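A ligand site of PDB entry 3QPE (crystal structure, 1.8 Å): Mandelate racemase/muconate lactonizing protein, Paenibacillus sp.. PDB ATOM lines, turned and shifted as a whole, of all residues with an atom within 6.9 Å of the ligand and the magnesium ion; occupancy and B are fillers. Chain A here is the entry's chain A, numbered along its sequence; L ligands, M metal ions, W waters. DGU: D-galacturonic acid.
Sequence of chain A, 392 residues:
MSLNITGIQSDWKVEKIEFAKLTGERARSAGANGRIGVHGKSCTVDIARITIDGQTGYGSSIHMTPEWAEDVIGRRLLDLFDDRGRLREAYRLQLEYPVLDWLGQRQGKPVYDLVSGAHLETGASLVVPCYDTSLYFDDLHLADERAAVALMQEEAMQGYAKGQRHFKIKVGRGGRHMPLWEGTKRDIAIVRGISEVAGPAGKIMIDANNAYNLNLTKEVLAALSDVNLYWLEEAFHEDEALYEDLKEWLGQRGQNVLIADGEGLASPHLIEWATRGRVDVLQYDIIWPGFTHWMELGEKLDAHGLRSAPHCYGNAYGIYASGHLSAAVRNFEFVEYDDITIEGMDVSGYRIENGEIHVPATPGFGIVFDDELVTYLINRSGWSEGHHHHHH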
ATOM      1  N   ALA A  32      34.566 -35.392  17.674  1.00  0.00           N
ATOM      2  CA  ALA A  32      35.133 -34.702  16.520  1.00  0.00           C
ATOM      3  C   ALA A  32      34.053 -34.214  15.562  1.00  0.00           C
ATOM      4  O   ALA A  32      32.892 -34.614  15.679  1.00  0.00           O
ATOM      5  CB  ALA A  32      36.098 -35.643  15.784  1.00  0.00           C
ATOM      6  N   ASN A  33      34.422 -33.314  14.653  1.00  0.00           N
ATOM      7  CA  ASN A  33      33.578 -32.953  13.526  1.00  0.00           C
ATOM      8  C   ASN A  33      34.347 -33.215  12.247  1.00  0.00           C
ATOM      9  O   ASN A  33      35.426 -33.811  12.294  1.00  0.00           O
ATOM     10  CB  ASN A  33      33.042 -31.496  13.605  1.00  0.00           C
ATOM     11  CG  ASN A  33      34.123 -30.450  13.389  1.00  0.00           C
ATOM     12  OD1 ASN A  33      35.230 -30.757  12.949  1.00  0.00           O
ATOM     13  ND2 ASN A  33      33.801 -29.198  13.716  1.00  0.00           N
ATOM     14  N   GLY A  34      33.791 -32.786  11.101  1.00  0.00           N
ATOM     15  CA  GLY A  34      34.369 -33.117   9.819  1.00  0.00           C
ATOM     16  C   GLY A  34      35.826 -32.713   9.631  1.00  0.00           C
ATOM     17  O   GLY A  34      36.560 -33.374   8.900  1.00  0.00           O
ATOM     18  N   ARG A  35      36.255 -31.638  10.297  1.00  0.00           N
ATOM     19  CA  ARG A  35      37.596 -31.091  10.057  1.00  0.00           C
ATOM     20  C   ARG A  35      38.592 -31.234  11.200  1.00  0.00           C
ATOM     21  O   ARG A  35      39.801 -31.238  10.950  1.00  0.00           O
ATOM     22  CB  ARG A  35      37.516 -29.616   9.653  1.00  0.00           C
ATOM     23  CG  ARG A  35      36.685 -28.727  10.600  1.00  0.00           C
ATOM     24  CD  ARG A  35      36.718 -27.249  10.149  1.00  0.00           C
ATOM     25  NE  ARG A  35      38.088 -26.737  10.103  1.00  0.00           N
ATOM     26  CZ  ARG A  35      38.714 -26.167  11.138  1.00  0.00           C
ATOM     27  NH1 ARG A  35      39.963 -25.759  10.996  1.00  0.00           N
ATOM     28  NH2 ARG A  35      38.089 -26.023  12.298  1.00  0.00           N
ATOM     29  N   ILE A  36      38.115 -31.295  12.434  1.00  0.00           N
ATOM     30  CA  ILE A  36      39.028 -31.301  13.582  1.00  0.00           C
ATOM     31  C   ILE A  36      38.632 -32.331  14.620  1.00  0.00           C
ATOM     32  O   ILE A  36      37.630 -33.031  14.476  1.00  0.00           O
ATOM     33  CB  ILE A  36      39.154 -29.898  14.239  1.00  0.00           C
ATOM     34  CG1 ILE A  36      37.811 -29.417  14.796  1.00  0.00           C
ATOM     35  CG2 ILE A  36      39.701 -28.884  13.225  1.00  0.00           C
ATOM     36  CD1 ILE A  36      37.899 -28.119  15.616  1.00  0.00           C
ATOM     37  N   GLY A  37      39.439 -32.431  15.671  1.00  0.00           N
ATOM     38  CA  GLY A  37      39.268 -33.465  16.674  1.00  0.00           C
ATOM     39  C   GLY A  37      38.198 -33.228  17.717  1.00  0.00           C
ATOM     40  O   GLY A  37      37.323 -32.375  17.569  1.00  0.00           O
ATOM     41  N   HIS A  39      35.973 -32.080  20.693  1.00  0.00           N
ATOM     42  CA  HIS A  39      35.755 -30.727  21.215  1.00  0.00           C
ATOM     43  C   HIS A  39      35.779 -30.698  22.729  1.00  0.00           C
ATOM     44  O   HIS A  39      36.144 -29.691  23.343  1.00  0.00           O
ATOM     45  CB  HIS A  39      34.444 -30.156  20.675  1.00  0.00           C
ATOM     46  CG  HIS A  39      34.497 -29.776  19.230  1.00  0.00           C
ATOM     47  ND1 HIS A  39      34.665 -30.702  18.219  1.00  0.00           N
ATOM     48  CD2 HIS A  39      34.404 -28.568  18.628  1.00  0.00           C
ATOM     49  CE1 HIS A  39      34.662 -30.080  17.057  1.00  0.00           C
ATOM     50  NE2 HIS A  39      34.509 -28.783  17.273  1.00  0.00           N
ATOM     51  N   TYR A 131      17.145 -25.991  18.299  1.00  0.00           N
ATOM     52  CA  TYR A 131      17.554 -27.326  17.869  1.00  0.00           C
ATOM     53  C   TYR A 131      18.782 -27.829  18.632  1.00  0.00           C
ATOM     54  O   TYR A 131      19.597 -27.036  19.128  1.00  0.00           O
ATOM     55  CB  TYR A 131      17.800 -27.361  16.360  1.00  0.00           C
ATOM     56  CG  TYR A 131      19.026 -26.627  15.884  1.00  0.00           C
ATOM     57  CD1 TYR A 131      20.288 -27.200  15.982  1.00  0.00           C
ATOM     58  CD2 TYR A 131      18.928 -25.372  15.310  1.00  0.00           C
ATOM     59  CE1 TYR A 131      21.417 -26.526  15.542  1.00  0.00           C
ATOM     60  CE2 TYR A 131      20.054 -24.696  14.856  1.00  0.00           C
ATOM     61  CZ  TYR A 131      21.286 -25.265  14.983  1.00  0.00           C
ATOM     62  OH  TYR A 131      22.396 -24.598  14.517  1.00  0.00           O
ATOM     63  N   THR A 133      22.289 -29.155  18.883  1.00  0.00           N
ATOM     64  CA  THR A 133      23.464 -29.049  18.027  1.00  0.00           C
ATOM     65  C   THR A 133      24.577 -30.007  18.445  1.00  0.00           C
ATOM     66  O   THR A 133      25.651 -30.032  17.850  1.00  0.00           O
ATOM     67  CB  THR A 133      23.988 -27.580  17.978  1.00  0.00           C
ATOM     68  OG1 THR A 133      24.850 -27.390  16.836  1.00  0.00           O
ATOM     69  CG2 THR A 133      24.769 -27.227  19.258  1.00  0.00           C
ATOM     70  N   TYR A 136      27.825 -34.783  17.581  1.00  0.00           N
ATOM     71  CA  TYR A 136      29.118 -34.828  16.921  1.00  0.00           C
ATOM     72  C   TYR A 136      29.471 -36.253  16.464  1.00  0.00           C
ATOM     73  O   TYR A 136      28.600 -37.114  16.438  1.00  0.00           O
ATOM     74  CB  TYR A 136      30.179 -34.232  17.857  1.00  0.00           C
ATOM     75  CG  TYR A 136      30.178 -32.726  17.774  1.00  0.00           C
ATOM     76  CD1 TYR A 136      29.067 -31.986  18.152  1.00  0.00           C
ATOM     77  CD2 TYR A 136      31.283 -32.032  17.262  1.00  0.00           C
ATOM     78  CE1 TYR A 136      29.062 -30.578  18.051  1.00  0.00           C
ATOM     79  CE2 TYR A 136      31.277 -30.643  17.144  1.00  0.00           C
ATOM     80  CZ  TYR A 136      30.173 -29.926  17.546  1.00  0.00           C
ATOM     81  OH  TYR A 136      30.178 -28.543  17.410  1.00  0.00           O
ATOM     82  N   LYS A 168      20.648 -31.177  14.820  1.00  0.00           N
ATOM     83  CA  LYS A 168      21.664 -30.965  13.794  1.00  0.00           C
ATOM     84  C   LYS A 168      22.782 -31.967  13.943  1.00  0.00           C
ATOM     85  O   LYS A 168      23.415 -32.076  14.987  1.00  0.00           O
ATOM     86  CB  LYS A 168      22.212 -29.535  13.815  1.00  0.00           C
ATOM     87  CG  LYS A 168      23.201 -29.259  12.685  1.00  0.00           C
ATOM     88  CD  LYS A 168      23.421 -27.765  12.479  1.00  0.00           C
ATOM     89  CE  LYS A 168      24.570 -27.234  13.330  1.00  0.00           C
ATOM     90  NZ  LYS A 168      24.538 -25.718  13.240  1.00  0.00           N
ATOM     91  N   LYS A 170      26.358 -33.731  12.827  1.00  0.00           N
ATOM     92  CA  LYS A 170      27.633 -33.593  12.150  1.00  0.00           C
ATOM     93  C   LYS A 170      27.829 -34.732  11.157  1.00  0.00           C
ATOM     94  O   LYS A 170      27.673 -35.891  11.521  1.00  0.00           O
ATOM     95  CB  LYS A 170      28.773 -33.600  13.168  1.00  0.00           C
ATOM     96  CG  LYS A 170      28.749 -32.404  14.102  1.00  0.00           C
ATOM     97  CD  LYS A 170      29.064 -31.112  13.333  1.00  0.00           C
ATOM     98  CE  LYS A 170      29.267 -29.916  14.282  1.00  0.00           C
ATOM     99  NZ  LYS A 170      28.241 -28.857  14.047  1.00  0.00           N
ATOM    100  N   ASP A 207      25.459 -30.994   8.980  1.00  0.00           N
ATOM    101  CA  ASP A 207      26.525 -29.995   8.952  1.00  0.00           C
ATOM    102  C   ASP A 207      27.837 -30.694   8.651  1.00  0.00           C
ATOM    103  O   ASP A 207      28.336 -31.474   9.459  1.00  0.00           O
ATOM    104  CB  ASP A 207      26.569 -29.201  10.272  1.00  0.00           C
ATOM    105  CG  ASP A 207      27.693 -28.189  10.320  1.00  0.00           C
ATOM    106  OD1 ASP A 207      28.494 -28.118   9.359  1.00  0.00           O
ATOM    107  OD2 ASP A 207      27.810 -27.485  11.359  1.00  0.00           O
ATOM    108  N   ALA A 208      28.380 -30.415   7.474  1.00  0.00           N
ATOM    109  CA  ALA A 208      29.551 -31.149   7.003  1.00  0.00           C
ATOM    110  C   ALA A 208      30.867 -30.532   7.434  1.00  0.00           C
ATOM    111  O   ALA A 208      31.930 -31.131   7.266  1.00  0.00           O
ATOM    112  CB  ALA A 208      29.495 -31.307   5.457  1.00  0.00           C
ATOM    113  N   ASN A 209      30.813 -29.327   7.988  1.00  0.00           N
ATOM    114  CA  ASN A 209      32.046 -28.594   8.276  1.00  0.00           C
ATOM    115  C   ASN A 209      33.016 -28.657   7.102  1.00  0.00           C
ATOM    116  O   ASN A 209      34.220 -28.870   7.271  1.00  0.00           O
ATOM    117  CB  ASN A 209      32.701 -29.039   9.580  1.00  0.00           C
ATOM    118  CG  ASN A 209      31.881 -28.651  10.799  1.00  0.00           C
ATOM    119  OD1 ASN A 209      31.166 -29.482  11.362  1.00  0.00           O
ATOM    120  ND2 ASN A 209      31.958 -27.389  11.208  1.00  0.00           N
ATOM    121  N   GLU A 233      24.198 -27.546   5.863  1.00  0.00           N
ATOM    122  CA  GLU A 233      25.084 -26.518   6.373  1.00  0.00           C
ATOM    123  C   GLU A 233      26.546 -26.802   6.047  1.00  0.00           C
ATOM    124  O   GLU A 233      27.057 -27.886   6.341  1.00  0.00           O
ATOM    125  CB  GLU A 233      24.883 -26.390   7.890  1.00  0.00           C
ATOM    126  CG  GLU A 233      25.967 -25.606   8.633  1.00  0.00           C
ATOM    127  CD  GLU A 233      25.553 -25.253  10.050  1.00  0.00           C
ATOM    128  OE1 GLU A 233      24.385 -25.426  10.430  1.00  0.00           O
ATOM    129  OE2 GLU A 233      26.411 -24.751  10.778  1.00  0.00           O
ATOM    130  N   GLU A 234      27.217 -25.844   5.429  1.00  0.00           N
ATOM    131  CA  GLU A 234      28.642 -25.967   5.095  1.00  0.00           C
ATOM    132  C   GLU A 234      29.039 -27.306   4.463  1.00  0.00           C
ATOM    133  O   GLU A 234      29.970 -27.966   4.922  1.00  0.00           O
ATOM    134  CB  GLU A 234      29.519 -25.682   6.317  1.00  0.00           C
ATOM    135  CG  GLU A 234      29.378 -24.257   6.852  1.00  0.00           C
ATOM    136  CD  GLU A 234      30.676 -23.742   7.507  1.00  0.00           C
ATOM    137  OE1 GLU A 234      31.165 -24.352   8.470  1.00  0.00           O
ATOM    138  OE2 GLU A 234      31.209 -22.732   7.049  1.00  0.00           O
ATOM    139  N   GLU A 263      29.308 -19.262   8.966  1.00  0.00           N
ATOM    140  CA  GLU A 263      30.140 -19.232  10.188  1.00  0.00           C
ATOM    141  C   GLU A 263      31.633 -19.061   9.876  1.00  0.00           C
ATOM    142  O   GLU A 263      32.078 -19.310   8.749  1.00  0.00           O
ATOM    143  CB  GLU A 263      29.907 -20.483  11.054  1.00  0.00           C
ATOM    144  CG  GLU A 263      30.624 -21.720  10.540  1.00  0.00           C
ATOM    145  CD  GLU A 263      30.250 -22.957  11.328  1.00  0.00           C
ATOM    146  OE1 GLU A 263      31.163 -23.630  11.869  1.00  0.00           O
ATOM    147  OE2 GLU A 263      29.039 -23.255  11.417  1.00  0.00           O
ATOM    148  N   GLN A 283      24.557 -17.626   8.705  1.00  0.00           N
ATOM    149  CA  GLN A 283      24.898 -18.161  10.029  1.00  0.00           C
ATOM    150  C   GLN A 283      26.074 -17.480  10.754  1.00  0.00           C
ATOM    151  O   GLN A 283      26.807 -18.121  11.520  1.00  0.00           O
ATOM    152  CB  GLN A 283      25.164 -19.674   9.886  1.00  0.00           C
ATOM    153  CG  GLN A 283      23.963 -20.423   9.363  1.00  0.00           C
ATOM    154  CD  GLN A 283      24.182 -21.926   9.348  1.00  0.00           C
ATOM    155  OE1 GLN A 283      25.122 -22.419   8.731  1.00  0.00           O
ATOM    156  NE2 GLN A 283      23.300 -22.658  10.011  1.00  0.00           N
ATOM    157  N   HIS A 311      25.030 -18.535  14.343  1.00  0.00           N
ATOM    158  CA  HIS A 311      25.849 -19.624  14.861  1.00  0.00           C
ATOM    159  C   HIS A 311      26.130 -19.375  16.339  1.00  0.00           C
ATOM    160  O   HIS A 311      26.406 -18.243  16.747  1.00  0.00           O
ATOM    161  CB  HIS A 311      27.181 -19.674  14.104  1.00  0.00           C
ATOM    162  CG  HIS A 311      28.210 -20.574  14.730  1.00  0.00           C
ATOM    163  ND1 HIS A 311      28.983 -20.194  15.804  1.00  0.00           N
ATOM    164  CD2 HIS A 311      28.605 -21.832  14.401  1.00  0.00           C
ATOM    165  CE1 HIS A 311      29.802 -21.174  16.123  1.00  0.00           C
ATOM    166  NE2 HIS A 311      29.590 -22.186  15.308  1.00  0.00           N
ATOM    167  N   CYS A 312      26.033 -20.427  17.134  1.00  0.00           N
ATOM    168  CA  CYS A 312      26.418 -20.333  18.534  1.00  0.00           C
ATOM    169  C   CYS A 312      26.956 -21.696  18.955  1.00  0.00           C
ATOM    170  O   CYS A 312      26.215 -22.673  19.018  1.00  0.00           O
ATOM    171  CB  CYS A 312      25.228 -19.947  19.403  1.00  0.00           C
ATOM    172  SG  CYS A 312      25.640 -19.819  21.152  1.00  0.00           S
ATOM    173  N   TYR A 313      28.245 -21.754  19.206  1.00  0.00           N
ATOM    174  CA  TYR A 313      28.864 -22.954  19.731  1.00  0.00           C
ATOM    175  C   TYR A 313      30.185 -22.511  20.329  1.00  0.00           C
ATOM    176  O   TYR A 313      30.924 -21.734  19.724  1.00  0.00           O
ATOM    177  CB  TYR A 313      29.091 -24.017  18.638  1.00  0.00           C
ATOM    178  CG  TYR A 313      29.408 -25.357  19.256  1.00  0.00           C
ATOM    179  CD1 TYR A 313      28.393 -26.188  19.696  1.00  0.00           C
ATOM    180  CD2 TYR A 313      30.712 -25.770  19.445  1.00  0.00           C
ATOM    181  CE1 TYR A 313      28.670 -27.428  20.306  1.00  0.00           C
ATOM    182  CE2 TYR A 313      31.009 -26.997  20.045  1.00  0.00           C
ATOM    183  CZ  TYR A 313      29.981 -27.815  20.467  1.00  0.00           C
ATOM    184  OH  TYR A 313      30.255 -29.034  21.065  1.00  0.00           O
ATOM    185  N   GLY A 314      30.462 -22.966  21.553  1.00  0.00           N
ATOM    186  CA  GLY A 314      31.688 -22.608  22.219  1.00  0.00           C
ATOM    187  C   GLY A 314      31.492 -21.479  23.211  1.00  0.00           C
ATOM    188  O   GLY A 314      32.430 -21.079  23.902  1.00  0.00           O
ATOM    189  N   GLU A 336      20.447 -22.052  18.248  1.00  0.00           N
ATOM    190  CA  GLU A 336      21.331 -23.209  18.254  1.00  0.00           C
ATOM    191  C   GLU A 336      21.645 -23.621  19.702  1.00  0.00           C
ATOM    192  O   GLU A 336      22.295 -22.877  20.432  1.00  0.00           O
ATOM    193  CB  GLU A 336      22.623 -22.934  17.466  1.00  0.00           C
ATOM    194  CG  GLU A 336      23.494 -24.180  17.304  1.00  0.00           C
ATOM    195  CD  GLU A 336      24.702 -23.965  16.403  1.00  0.00           C
ATOM    196  OE1 GLU A 336      24.922 -22.822  15.957  1.00  0.00           O
ATOM    197  OE2 GLU A 336      25.429 -24.943  16.145  1.00  0.00           O
HETATM  198  O1  DGU L   1      34.009 -24.123  16.990  1.00  0.00           O
HETATM  199  O2  DGU L   1      34.264 -26.611  15.685  1.00  0.00           O
HETATM  200  O5  DGU L   1      30.110 -25.780  12.868  1.00  0.00           O
HETATM  201  O6B DGU L   1      27.437 -25.162  13.390  1.00  0.00           O
HETATM  202  C1  DGU L   1      33.056 -24.637  16.391  1.00  0.00           C
HETATM  203  C2  DGU L   1      32.971 -26.152  16.127  1.00  0.00           C
HETATM  204  C3  DGU L   1      31.909 -26.518  15.060  1.00  0.00           C
HETATM  205  C4  DGU L   1      30.530 -25.842  15.277  1.00  0.00           C
HETATM  206  C5  DGU L   1      29.530 -26.083  14.138  1.00  0.00           C
HETATM  207  C6  DGU L   1      28.182 -25.359  14.384  1.00  0.00           C
HETATM  208  O3  DGU L   1      31.724 -27.941  15.048  1.00  0.00           O
HETATM  209  O4  DGU L   1      30.719 -24.430  15.374  1.00  0.00           O
HETATM  210  O6A DGU L   1      27.945 -25.025  15.564  1.00  0.00           O
HETATM  211 MG    MG M   1      28.314 -25.339  11.376  1.00  0.00          MG
HETATM  212  O   HOH W   1      25.317 -22.660  13.048  1.00  0.00           O
HETATM  213  O   HOH W   2      35.383 -26.492  13.072  1.00  0.00           O
HETATM  214  O   HOH W   3      27.516 -27.714  16.746  1.00  0.00           O
HETATM  215  O   HOH W   4      29.719 -25.710   9.733  1.00  0.00           O
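The side-chain carboxylate of Glu 336 lies close to an oxygen (O6A) of the ligand.
NZ of Lys 170 lies close to O6B of the ligand (3.8 Å).
NE2 of His 311 lies within hydrogen-bond range of O4 of the ligand, 2.5 Å away.
The side-chain amide nitrogen (ND2) of Asn 209 lies close to an oxygen (O5) of the ligand (3.0 Å).
ND2 of Asn 33 is in hydrogen-bond range of O3 of the ligand (2.8 Å).
A ring nitrogen (NE2) of His 39 sits at hydrogen-bond distance from an oxygen (O2) of the ligand (2.7 Å).
The side-chain hydroxyl (OH) of Tyr 136 lies within hydrogen-bond range of an oxygen (O3) of the ligand (2.9 Å).
The side-chain amino group of Lys 168 lies close to an oxygen (O6B) of the ligand (3.0 Å).
N of Asn 209 sits at hydrogen-bond distance from OD1 of Asp 207, at 3.0 Å.
The side-chain amino group (NZ) of Lys 168 is in salt-bridge range of the side-chain carboxylate (OE2) of Glu 336 (3.1 Å).
OE1 of Glu 233 lies within salt-bridge range of NZ of Lys 168.
The backbone NH of Ile 36 is in hydrogen-bond range of the side-chain amide oxygen of Asn 33, 3.0 Å away.
OE1 of Glu 233 is in hydrogen-bond range of NE2 of Gln 283 (3.0 Å).
O of Gly 37 is in hydrogen-bond range of ND1 of His 39, at 3.2 Å.
The backbone NH (N) of Ala 208 sits at hydrogen-bond distance from the backbone carbonyl oxygen (O) of Glu 233, at 3.1 Å.
O of Glu 234 lies within hydrogen-bond range of N of Asn 209 (3.5 Å).
Residues that only touch the ligand: Tyr 313 (3.4 Å) and Ile 36 (3.9 Å).
Hydrophobic or aromatic side chains that line the ligand: Ile 36, His 39, Tyr 136, His 311 and Tyr 313.
13 residues have an atom within 4 Å of the ligand: Asn 33, Ile 36, His 39, Tyr 136, Lys 168, Lys 170, Asp 207, Asn 209, Glu 233, Glu 263, His 311, Tyr 313 and Glu 336.
Water W4 lies within hydrogen-bond range of OD1 of Asp 207 (2.7 Å), ND2 of Asn 209 (3.2 Å) and OE1 of Glu 263 (3.3 Å).
Water W2 lies within hydrogen-bond range of an oxygen (O2) of the ligand (2.8 Å), the guanidinium group (NH2) of Arg 35 (2.9 Å) and the side-chain amide nitrogen (ND2) of Asn 33 (3.2 Å).
Water W3 lies within hydrogen-bond range of OG1 of Thr 133 (2.7 Å), OH of Tyr 136 (2.9 Å), O6A of the ligand (3.0 Å) and NZ of Lys 170 (3.0 Å).
Water W1 bridges the side-chain carboxylate of Glu 336 and the side-chain amino group of Lys 168.
Three residues have an atom within 4 Å of the magnesium ion: Asp 207, Glu 233 and Glu 263.
The nearest printed residue that does not touch the magnesium ion is Asn 209 (4.2 Å).
The magnesium ion is bound by OE2 of Glu 233 (2.1 Å), water W4 (2.2 Å), O6B of the ligand (2.2 Å), OD2 of Asp 207 (2.2 Å), OE2 of Glu 263 (2.2 Å) and O5 of the ligand (2.4 Å).
The magnesium ion has six donor atoms within binding distance.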
